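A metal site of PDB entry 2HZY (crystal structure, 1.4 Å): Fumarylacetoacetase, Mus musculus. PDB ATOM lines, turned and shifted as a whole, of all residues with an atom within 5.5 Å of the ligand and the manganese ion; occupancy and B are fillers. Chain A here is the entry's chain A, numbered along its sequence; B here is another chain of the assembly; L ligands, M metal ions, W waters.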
ATOM      1  N   TYR A 126     -28.219 -19.458  -8.715  1.00  0.00           N
ATOM      2  CA  TYR A 126     -28.652 -20.470  -7.763  1.00  0.00           C
ATOM      3  C   TYR A 126     -28.567 -19.864  -6.398  1.00  0.00           C
ATOM      4  O   TYR A 126     -27.580 -19.220  -6.014  1.00  0.00           O
ATOM      5  CB  TYR A 126     -27.737 -21.715  -7.932  1.00  0.00           C
ATOM      6  CG  TYR A 126     -27.573 -22.622  -6.725  1.00  0.00           C
ATOM      7  CD1 TYR A 126     -26.303 -22.964  -6.290  1.00  0.00           C
ATOM      8  CD2 TYR A 126     -28.678 -23.095  -6.022  1.00  0.00           C
ATOM      9  CE1 TYR A 126     -26.137 -23.786  -5.161  1.00  0.00           C
ATOM     10  CE2 TYR A 126     -28.525 -23.862  -4.894  1.00  0.00           C
ATOM     11  CZ  TYR A 126     -27.247 -24.218  -4.503  1.00  0.00           C
ATOM     12  OH  TYR A 126     -27.073 -24.906  -3.311  1.00  0.00           O
ATOM     13  N   ASP A 128     -29.329 -20.939  -2.197  1.00  0.00           N
ATOM     14  CA  ASP A 128     -29.632 -22.022  -1.241  1.00  0.00           C
ATOM     15  C   ASP A 128     -30.214 -21.358   0.010  1.00  0.00           C
ATOM     16  O   ASP A 128     -29.583 -20.512   0.650  1.00  0.00           O
ATOM     17  CB  ASP A 128     -28.376 -22.822  -0.933  1.00  0.00           C
ATOM     18  CG  ASP A 128     -28.619 -24.079  -0.151  1.00  0.00           C
ATOM     19  OD1 ASP A 128     -29.757 -24.612  -0.304  1.00  0.00           O
ATOM     20  OD2 ASP A 128     -27.730 -24.587   0.565  1.00  0.00           O
ATOM     21  N   PHE A 129     -31.432 -21.761   0.357  1.00  0.00           N
ATOM     22  CA  PHE A 129     -32.059 -21.311   1.612  1.00  0.00           C
ATOM     23  C   PHE A 129     -31.654 -22.214   2.770  1.00  0.00           C
ATOM     24  O   PHE A 129     -30.769 -23.072   2.652  1.00  0.00           O
ATOM     25  CB  PHE A 129     -33.589 -21.160   1.397  1.00  0.00           C
ATOM     26  CG  PHE A 129     -33.939 -19.964   0.550  1.00  0.00           C
ATOM     27  CD1 PHE A 129     -34.086 -20.040  -0.834  1.00  0.00           C
ATOM     28  CD2 PHE A 129     -34.060 -18.720   1.185  1.00  0.00           C
ATOM     29  CE1 PHE A 129     -34.345 -18.913  -1.580  1.00  0.00           C
ATOM     30  CE2 PHE A 129     -34.352 -17.586   0.442  1.00  0.00           C
ATOM     31  CZ  PHE A 129     -34.504 -17.678  -0.925  1.00  0.00           C
ATOM     32  N   TYR A 130     -32.280 -22.000   3.925  1.00  0.00           N
ATOM     33  CA  TYR A 130     -31.840 -22.593   5.181  1.00  0.00           C
ATOM     34  C   TYR A 130     -33.096 -22.835   6.014  1.00  0.00           C
ATOM     35  O   TYR A 130     -33.132 -22.589   7.237  1.00  0.00           O
ATOM     36  CB  TYR A 130     -30.882 -21.583   5.845  1.00  0.00           C
ATOM     37  CG  TYR A 130     -30.137 -21.932   7.095  1.00  0.00           C
ATOM     38  CD1 TYR A 130     -29.586 -23.191   7.296  1.00  0.00           C
ATOM     39  CD2 TYR A 130     -29.906 -20.964   8.057  1.00  0.00           C
ATOM     40  CE1 TYR A 130     -28.814 -23.473   8.388  1.00  0.00           C
ATOM     41  CE2 TYR A 130     -29.156 -21.245   9.145  1.00  0.00           C
ATOM     42  CZ  TYR A 130     -28.615 -22.471   9.323  1.00  0.00           C
ATOM     43  OH  TYR A 130     -27.816 -22.878  10.407  1.00  0.00           O
ATOM     44  N   SER A 131     -34.121 -23.374   5.350  1.00  0.00           N
ATOM     45  CA  SER A 131     -35.491 -23.232   5.888  1.00  0.00           C
ATOM     46  C   SER A 131     -36.016 -24.384   6.759  1.00  0.00           C
ATOM     47  O   SER A 131     -37.191 -24.325   7.144  1.00  0.00           O
ATOM     48  CB  SER A 131     -36.492 -22.910   4.768  1.00  0.00           C
ATOM     49  OG  SER A 131     -36.136 -21.673   4.110  1.00  0.00           O
ATOM     50  N   HIS A 135     -32.780 -28.522  10.957  1.00  0.00           N
ATOM     51  CA  HIS A 135     -31.439 -28.438  10.437  1.00  0.00           C
ATOM     52  C   HIS A 135     -30.681 -27.246  10.984  1.00  0.00           C
ATOM     53  O   HIS A 135     -29.551 -27.389  11.408  1.00  0.00           O
ATOM     54  CB  HIS A 135     -31.445 -28.400   8.903  1.00  0.00           C
ATOM     55  CG  HIS A 135     -30.100 -28.150   8.308  1.00  0.00           C
ATOM     56  ND1 HIS A 135     -29.098 -29.104   8.205  1.00  0.00           N
ATOM     57  CD2 HIS A 135     -29.603 -27.022   7.741  1.00  0.00           C
ATOM     58  CE1 HIS A 135     -28.024 -28.546   7.657  1.00  0.00           C
ATOM     59  NE2 HIS A 135     -28.299 -27.276   7.375  1.00  0.00           N
ATOM     60  N   ALA A 136     -31.286 -26.054  10.893  1.00  0.00           N
ATOM     61  CA  ALA A 136     -30.646 -24.874  11.468  1.00  0.00           C
ATOM     62  C   ALA A 136     -30.365 -25.002  12.970  1.00  0.00           C
ATOM     63  O   ALA A 136     -29.302 -24.579  13.395  1.00  0.00           O
ATOM     64  CB  ALA A 136     -31.512 -23.605  11.174  1.00  0.00           C
ATOM     65  N   VAL A 139     -27.340 -27.515  13.377  1.00  0.00           N
ATOM     66  CA  VAL A 139     -26.079 -26.876  13.060  1.00  0.00           C
ATOM     67  C   VAL A 139     -25.775 -25.948  14.280  1.00  0.00           C
ATOM     68  O   VAL A 139     -24.673 -25.975  14.857  1.00  0.00           O
ATOM     69  CB  VAL A 139     -26.052 -26.244  11.642  1.00  0.00           C
ATOM     70  CG1 VAL A 139     -24.735 -25.546  11.387  1.00  0.00           C
ATOM     71  CG2 VAL A 139     -26.230 -27.326  10.560  1.00  0.00           C
ATOM     72  N   GLY A 140     -26.796 -25.211  14.735  1.00  0.00           N
ATOM     73  CA  GLY A 140     -26.612 -24.342  15.886  1.00  0.00           C
ATOM     74  C   GLY A 140     -26.182 -25.069  17.152  1.00  0.00           C
ATOM     75  O   GLY A 140     -25.285 -24.564  17.883  1.00  0.00           O
ATOM     76  N   PHE A 143     -22.514 -26.165  16.786  1.00  0.00           N
ATOM     77  CA  PHE A 143     -21.495 -25.143  16.558  1.00  0.00           C
ATOM     78  C   PHE A 143     -21.467 -24.009  17.611  1.00  0.00           C
ATOM     79  O   PHE A 143     -20.438 -23.377  17.820  1.00  0.00           O
ATOM     80  CB  PHE A 143     -21.803 -24.441  15.231  1.00  0.00           C
ATOM     81  CG  PHE A 143     -21.297 -25.115  14.011  1.00  0.00           C
ATOM     82  CD1 PHE A 143     -21.126 -24.331  12.859  1.00  0.00           C
ATOM     83  CD2 PHE A 143     -21.043 -26.482  13.952  1.00  0.00           C
ATOM     84  CE1 PHE A 143     -20.668 -24.913  11.668  1.00  0.00           C
ATOM     85  CE2 PHE A 143     -20.569 -27.089  12.760  1.00  0.00           C
ATOM     86  CZ  PHE A 143     -20.388 -26.295  11.629  1.00  0.00           C
ATOM     87  N   ARG A 144     -22.622 -23.735  18.209  1.00  0.00           N
ATOM     88  CA  ARG A 144     -22.790 -22.506  18.943  1.00  0.00           C
ATOM     89  C   ARG A 144     -23.434 -22.862  20.314  1.00  0.00           C
ATOM     90  O   ARG A 144     -23.466 -22.030  21.243  1.00  0.00           O
ATOM     91  CB  ARG A 144     -23.630 -21.467  18.104  1.00  0.00           C
ATOM     92  CG  ARG A 144     -22.980 -21.004  16.648  1.00  0.00           C
ATOM     93  CD  ARG A 144     -23.949 -20.243  15.591  1.00  0.00           C
ATOM     94  NE  ARG A 144     -23.348 -20.239  14.225  1.00  0.00           N
ATOM     95  CZ  ARG A 144     -23.843 -20.787  13.074  1.00  0.00           C
ATOM     96  NH1 ARG A 144     -25.052 -21.334  12.988  1.00  0.00           N
ATOM     97  NH2 ARG A 144     -23.053 -20.780  11.980  1.00  0.00           N
ATOM     98  N   TYR A 161     -28.327 -17.891   0.938  1.00  0.00           N
ATOM     99  CA  TYR A 161     -27.087 -17.294   0.384  1.00  0.00           C
ATOM    100  C   TYR A 161     -27.039 -17.640  -1.083  1.00  0.00           C
ATOM    101  O   TYR A 161     -27.694 -18.609  -1.562  1.00  0.00           O
ATOM    102  CB  TYR A 161     -25.828 -17.824   1.124  1.00  0.00           C
ATOM    103  CG  TYR A 161     -25.601 -19.318   0.948  1.00  0.00           C
ATOM    104  CD1 TYR A 161     -24.611 -19.793   0.075  1.00  0.00           C
ATOM    105  CD2 TYR A 161     -26.388 -20.240   1.642  1.00  0.00           C
ATOM    106  CE1 TYR A 161     -24.448 -21.173  -0.158  1.00  0.00           C
ATOM    107  CE2 TYR A 161     -26.206 -21.643   1.438  1.00  0.00           C
ATOM    108  CZ  TYR A 161     -25.229 -22.071   0.541  1.00  0.00           C
ATOM    109  OH  TYR A 161     -25.096 -23.423   0.289  1.00  0.00           O
ATOM    110  N   GLU A 201     -25.970 -33.117   1.485  1.00  0.00           N
ATOM    111  CA  GLU A 201     -27.093 -32.399   2.080  1.00  0.00           C
ATOM    112  C   GLU A 201     -28.317 -32.691   1.273  1.00  0.00           C
ATOM    113  O   GLU A 201     -28.404 -32.332   0.092  1.00  0.00           O
ATOM    114  CB  GLU A 201     -26.893 -30.877   2.085  1.00  0.00           C
ATOM    115  CG  GLU A 201     -25.854 -30.380   3.107  1.00  0.00           C
ATOM    116  CD  GLU A 201     -25.917 -28.849   3.261  1.00  0.00           C
ATOM    117  OE1 GLU A 201     -25.608 -28.331   4.350  1.00  0.00           O
ATOM    118  OE2 GLU A 201     -26.287 -28.147   2.340  1.00  0.00           O
ATOM    119  N   GLU A 203     -31.661 -31.858  -0.120  1.00  0.00           N
ATOM    120  CA  GLU A 203     -32.483 -30.656  -0.351  1.00  0.00           C
ATOM    121  C   GLU A 203     -33.444 -30.920  -1.482  1.00  0.00           C
ATOM    122  O   GLU A 203     -33.330 -31.907  -2.204  1.00  0.00           O
ATOM    123  CB  GLU A 203     -31.575 -29.454  -0.727  1.00  0.00           C
ATOM    124  CG  GLU A 203     -30.470 -29.239   0.311  1.00  0.00           C
ATOM    125  CD  GLU A 203     -29.858 -27.862   0.286  1.00  0.00           C
ATOM    126  OE1 GLU A 203     -30.611 -26.885   0.025  1.00  0.00           O
ATOM    127  OE2 GLU A 203     -28.635 -27.734   0.547  1.00  0.00           O
ATOM    128  N   ASP A 235     -26.550 -30.896  -1.931  1.00  0.00           N
ATOM    129  CA  ASP A 235     -25.594 -29.803  -1.799  1.00  0.00           C
ATOM    130  C   ASP A 235     -24.330 -30.356  -1.137  1.00  0.00           C
ATOM    131  O   ASP A 235     -24.127 -30.172   0.062  1.00  0.00           O
ATOM    132  CB  ASP A 235     -26.244 -28.648  -0.999  1.00  0.00           C
ATOM    133  CG  ASP A 235     -25.376 -27.438  -0.857  1.00  0.00           C
ATOM    134  OD1 ASP A 235     -24.355 -27.306  -1.615  1.00  0.00           O
ATOM    135  OD2 ASP A 235     -25.688 -26.570   0.044  1.00  0.00           O
ATOM    136  N   SER A 237     -20.891 -30.789   0.499  1.00  0.00           N
ATOM    137  CA  SER A 237     -20.299 -29.797   1.419  1.00  0.00           C
ATOM    138  C   SER A 237     -18.981 -30.342   1.946  1.00  0.00           C
ATOM    139  O   SER A 237     -18.854 -31.545   2.242  1.00  0.00           O
ATOM    140  CB  SER A 237     -21.263 -29.501   2.593  1.00  0.00           C
ATOM    141  OG  SER A 237     -22.511 -29.033   2.070  1.00  0.00           O
ATOM    142  N   ARG A 239     -16.965 -29.766   5.113  1.00  0.00           N
ATOM    143  CA  ARG A 239     -17.312 -29.055   6.356  1.00  0.00           C
ATOM    144  C   ARG A 239     -16.112 -28.381   7.013  1.00  0.00           C
ATOM    145  O   ARG A 239     -16.266 -27.375   7.696  1.00  0.00           O
ATOM    146  CB  ARG A 239     -17.997 -29.971   7.366  1.00  0.00           C
ATOM    147  CG  ARG A 239     -19.307 -30.570   6.880  1.00  0.00           C
ATOM    148  CD  ARG A 239     -20.322 -29.544   6.432  1.00  0.00           C
ATOM    149  NE  ARG A 239     -21.655 -30.138   6.262  1.00  0.00           N
ATOM    150  CZ  ARG A 239     -22.738 -29.418   6.033  1.00  0.00           C
ATOM    151  NH1 ARG A 239     -22.670 -28.090   5.951  1.00  0.00           N
ATOM    152  NH2 ARG A 239     -23.919 -30.003   5.931  1.00  0.00           N
ATOM    153  N   GLN A 242     -15.496 -25.310   4.937  1.00  0.00           N
ATOM    154  CA  GLN A 242     -16.571 -24.401   5.272  1.00  0.00           C
ATOM    155  C   GLN A 242     -16.353 -23.679   6.586  1.00  0.00           C
ATOM    156  O   GLN A 242     -16.491 -22.451   6.661  1.00  0.00           O
ATOM    157  CB  GLN A 242     -17.892 -25.174   5.283  1.00  0.00           C
ATOM    158  CG  GLN A 242     -19.133 -24.294   5.483  1.00  0.00           C
ATOM    159  CD  GLN A 242     -20.437 -25.080   5.435  1.00  0.00           C
ATOM    160  OE1 GLN A 242     -20.458 -26.263   5.012  1.00  0.00           O
ATOM    161  NE2 GLN A 242     -21.514 -24.474   5.861  1.00  0.00           N
ATOM    162  N   TYR A 246     -15.991 -19.367   6.550  1.00  0.00           N
ATOM    163  CA  TYR A 246     -17.319 -18.791   6.329  1.00  0.00           C
ATOM    164  C   TYR A 246     -17.596 -17.521   7.094  1.00  0.00           C
ATOM    165  O   TYR A 246     -18.606 -16.873   6.819  1.00  0.00           O
ATOM    166  CB  TYR A 246     -18.459 -19.827   6.557  1.00  0.00           C
ATOM    167  CG  TYR A 246     -18.901 -19.952   7.983  1.00  0.00           C
ATOM    168  CD1 TYR A 246     -20.091 -19.343   8.421  1.00  0.00           C
ATOM    169  CD2 TYR A 246     -18.133 -20.634   8.901  1.00  0.00           C
ATOM    170  CE1 TYR A 246     -20.489 -19.431   9.769  1.00  0.00           C
ATOM    171  CE2 TYR A 246     -18.517 -20.741  10.241  1.00  0.00           C
ATOM    172  CZ  TYR A 246     -19.692 -20.165  10.659  1.00  0.00           C
ATOM    173  OH  TYR A 246     -20.064 -20.277  12.005  1.00  0.00           O
ATOM    174  N   PRO A 251     -20.802 -19.367   3.413  1.00  0.00           N
ATOM    175  CA  PRO A 251     -20.163 -20.554   2.808  1.00  0.00           C
ATOM    176  C   PRO A 251     -19.753 -20.247   1.374  1.00  0.00           C
ATOM    177  O   PRO A 251     -20.448 -19.505   0.651  1.00  0.00           O
ATOM    178  CB  PRO A 251     -21.273 -21.604   2.834  1.00  0.00           C
ATOM    179  CG  PRO A 251     -22.523 -20.937   3.233  1.00  0.00           C
ATOM    180  CD  PRO A 251     -22.219 -19.564   3.705  1.00  0.00           C
ATOM    181  N   LYS A 255     -18.920 -25.203  -0.438  1.00  0.00           N
ATOM    182  CA  LYS A 255     -20.111 -25.638  -1.161  1.00  0.00           C
ATOM    183  C   LYS A 255     -19.896 -25.727  -2.648  1.00  0.00           C
ATOM    184  O   LYS A 255     -20.660 -26.468  -3.330  1.00  0.00           O
ATOM    185  CB  LYS A 255     -21.263 -24.606  -0.967  1.00  0.00           C
ATOM    186  CG  LYS A 255     -21.681 -24.428   0.459  1.00  0.00           C
ATOM    187  CD  LYS A 255     -22.307 -25.674   1.020  1.00  0.00           C
ATOM    188  CE  LYS A 255     -22.956 -25.364   2.336  1.00  0.00           C
ATOM    189  NZ  LYS A 255     -23.663 -26.593   2.855  1.00  0.00           N
ATOM    190  N   GLY A 351     -32.899 -25.541   1.369  1.00  0.00           N
ATOM    191  CA  GLY A 351     -32.149 -25.838   2.593  1.00  0.00           C
ATOM    192  C   GLY A 351     -32.173 -27.345   2.860  1.00  0.00           C
ATOM    193  O   GLY A 351     -33.008 -28.097   2.330  1.00  0.00           O
ATOM    194  N   THR A 352     -31.250 -27.798   3.696  1.00  0.00           N
ATOM    195  CA  THR A 352     -31.199 -29.195   4.105  1.00  0.00           C
ATOM    196  C   THR A 352     -32.444 -29.568   4.860  1.00  0.00           C
ATOM    197  O   THR A 352     -32.873 -28.879   5.821  1.00  0.00           O
ATOM    198  CB  THR A 352     -29.929 -29.407   4.931  1.00  0.00           C
ATOM    199  OG1 THR A 352     -28.803 -29.093   4.107  1.00  0.00           O
ATOM    200  CG2 THR A 352     -29.781 -30.882   5.390  1.00  0.00           C
ATOM    201  N   PRO B 248     -25.860 -16.380   9.693  1.00  0.00           N
ATOM    202  CA  PRO B 248     -24.453 -16.735   9.464  1.00  0.00           C
ATOM    203  C   PRO B 248     -24.086 -16.949   7.981  1.00  0.00           C
ATOM    204  O   PRO B 248     -22.929 -17.348   7.740  1.00  0.00           O
ATOM    205  CB  PRO B 248     -24.392 -18.090  10.196  1.00  0.00           C
ATOM    206  CG  PRO B 248     -25.750 -18.734   9.975  1.00  0.00           C
ATOM    207  CD  PRO B 248     -26.722 -17.573   9.785  1.00  0.00           C
ATOM    208  N   LEU B 249     -24.985 -16.749   7.036  1.00  0.00           N
ATOM    209  CA  LEU B 249     -24.712 -17.206   5.672  1.00  0.00           C
ATOM    210  C   LEU B 249     -24.263 -16.125   4.721  1.00  0.00           C
ATOM    211  O   LEU B 249     -24.011 -16.435   3.536  1.00  0.00           O
ATOM    212  CB  LEU B 249     -25.917 -17.967   5.063  1.00  0.00           C
ATOM    213  CG  LEU B 249     -26.334 -19.181   5.941  1.00  0.00           C
ATOM    214  CD1 LEU B 249     -27.456 -19.975   5.275  1.00  0.00           C
ATOM    215  CD2 LEU B 249     -25.153 -20.125   6.380  1.00  0.00           C
HETATM  216  O1  LIG L   1     -23.475 -22.133   9.388  1.00  0.00           O
HETATM  217  C1  LIG L   1     -24.695 -22.546   9.451  1.00  0.00           C
HETATM  218  O2  LIG L   1     -25.420 -22.211  10.374  1.00  0.00           O
HETATM  219  C2  LIG L   1     -25.332 -23.451   8.416  1.00  0.00           C
HETATM  220  C3  LIG L   1     -24.650 -23.868   7.338  1.00  0.00           C
HETATM  221  P1  LIG L   1     -25.288 -24.897   6.069  1.00  0.00           P
HETATM  222  O3  LIG L   1     -24.111 -25.708   5.566  1.00  0.00           O
HETATM  223  O4  LIG L   1     -26.541 -25.627   6.441  1.00  0.00           O
HETATM  224  C4  LIG L   1     -25.734 -23.718   4.756  1.00  0.00           C
HETATM  225  C5  LIG L   1     -26.575 -24.401   3.738  1.00  0.00           C
HETATM  226  O5  LIG L   1     -26.125 -25.113   2.819  1.00  0.00           O
HETATM  227  C6  LIG L   1     -28.096 -24.208   3.833  1.00  0.00           C
HETATM  228  C7  LIG L   1     -28.843 -25.542   3.928  1.00  0.00           C
HETATM  229  O6  LIG L   1     -28.579 -26.440   3.084  1.00  0.00           O
HETATM  230  O7  LIG L   1     -29.708 -25.682   4.847  1.00  0.00           O
HETATM  231 MN    MN M   1     -27.235 -26.466   1.487  1.00  0.00          MN
HETATM  232  O   HOH W   1     -21.373 -22.211   7.481  1.00  0.00           O
HETATM  233  O   HOH W   2     -32.390 -26.073   6.142  1.00  0.00           O
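Tyr 161 touches the manganese ion. Lys 255 touches the manganese ion (NZ to MN, 3.8 Å). The nearest printed residue that does not touch the manganese ion is Thr 352 (4.03 Å).
Water W1 bridges the side-chain amide nitrogen (NE2) of Gln 242 and an oxygen (O1) of the ligand. Water W2 lies within hydrogen-bond range of the backbone carbonyl oxygen of Thr 352, an oxygen (O7) of the ligand and the backbone NH of Ser 131.
The manganese ion is bound by O6 of the ligand (2.1 Å), OE2 of Glu 201 (2.1 Å), OE2 of Glu 203 (2.1 Å), OD2 of Asp 235 (2.1 Å), OD2 of Asp 128 (2.2 Å) and O5 of the ligand (2.2 Å). The manganese ion has six donor atoms within binding distance.
The guanidinium group (NH2) of Arg 239 is in salt-bridge range of the side-chain carboxylate (OE1) of Glu 201. OG1 of Thr 352 sits close to OE1 of Glu 201 (3.3 Å). OE1 of Glu 201 lies within salt-bridge range of NZ of Lys 255 (3.0 Å). The side-chain carboxylate (OE1) of Glu 203 is in hydrogen-bond range of the backbone NH (N) of Gly 351 (3.0 Å). The side-chain carboxylate (OD2) of Asp 235 sits close to the side-chain hydroxyl (OH) of Tyr 161, 3.2 Å away. O of Tyr 161 sits at hydrogen-bond distance from N of Asp 128, at 2.9 Å. The side-chain hydroxyl (OH) of Tyr 246 sits at hydrogen-bond distance from the guanidinium group (NH2) of Arg 144, at 3.0 Å. The guanidinium group (NH1) of Arg 239 lies within hydrogen-bond range of the side-chain amide oxygen (OE1) of Gln 242.
Phe 129 touches the ligand. Val 139 touches the ligand. CA of Gly 351 touches O7 of the ligand (3.3 Å). Pro 248 of chain B touches the ligand. Leu 249 of chain B touches the ligand (CD2 to C3, 3.9 Å).
O2 of the ligand lies within hydrogen-bond range of OH of Tyr 130 (2.5 Å). NE2 of His 135 is in hydrogen-bond range of O4 of the ligand (2.6 Å). The guanidinium group (NH1) of Arg 144 is in salt-bridge range of an oxygen (O2) of the ligand (2.8 Å). An oxygen (O3) of the ligand is in salt-bridge range of the guanidinium group (NH1) of Arg 239 (2.8 Å). An oxygen (O7) of the ligand is in hydrogen-bond range of the backbone NH (N) of Thr 352, 2.9 Å away. OG1 of Thr 352 sits close to O6 of the ligand (2.9 Å). An oxygen (O3) of the ligand is in salt-bridge range of the side-chain amino group (NZ) of Lys 255. O3 of the ligand lies within hydrogen-bond range of NE2 of Gln 242 (2.9 Å). An oxygen (O5) of the ligand lies close to the side-chain hydroxyl (OH) of Tyr 161, 3.2 Å away.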
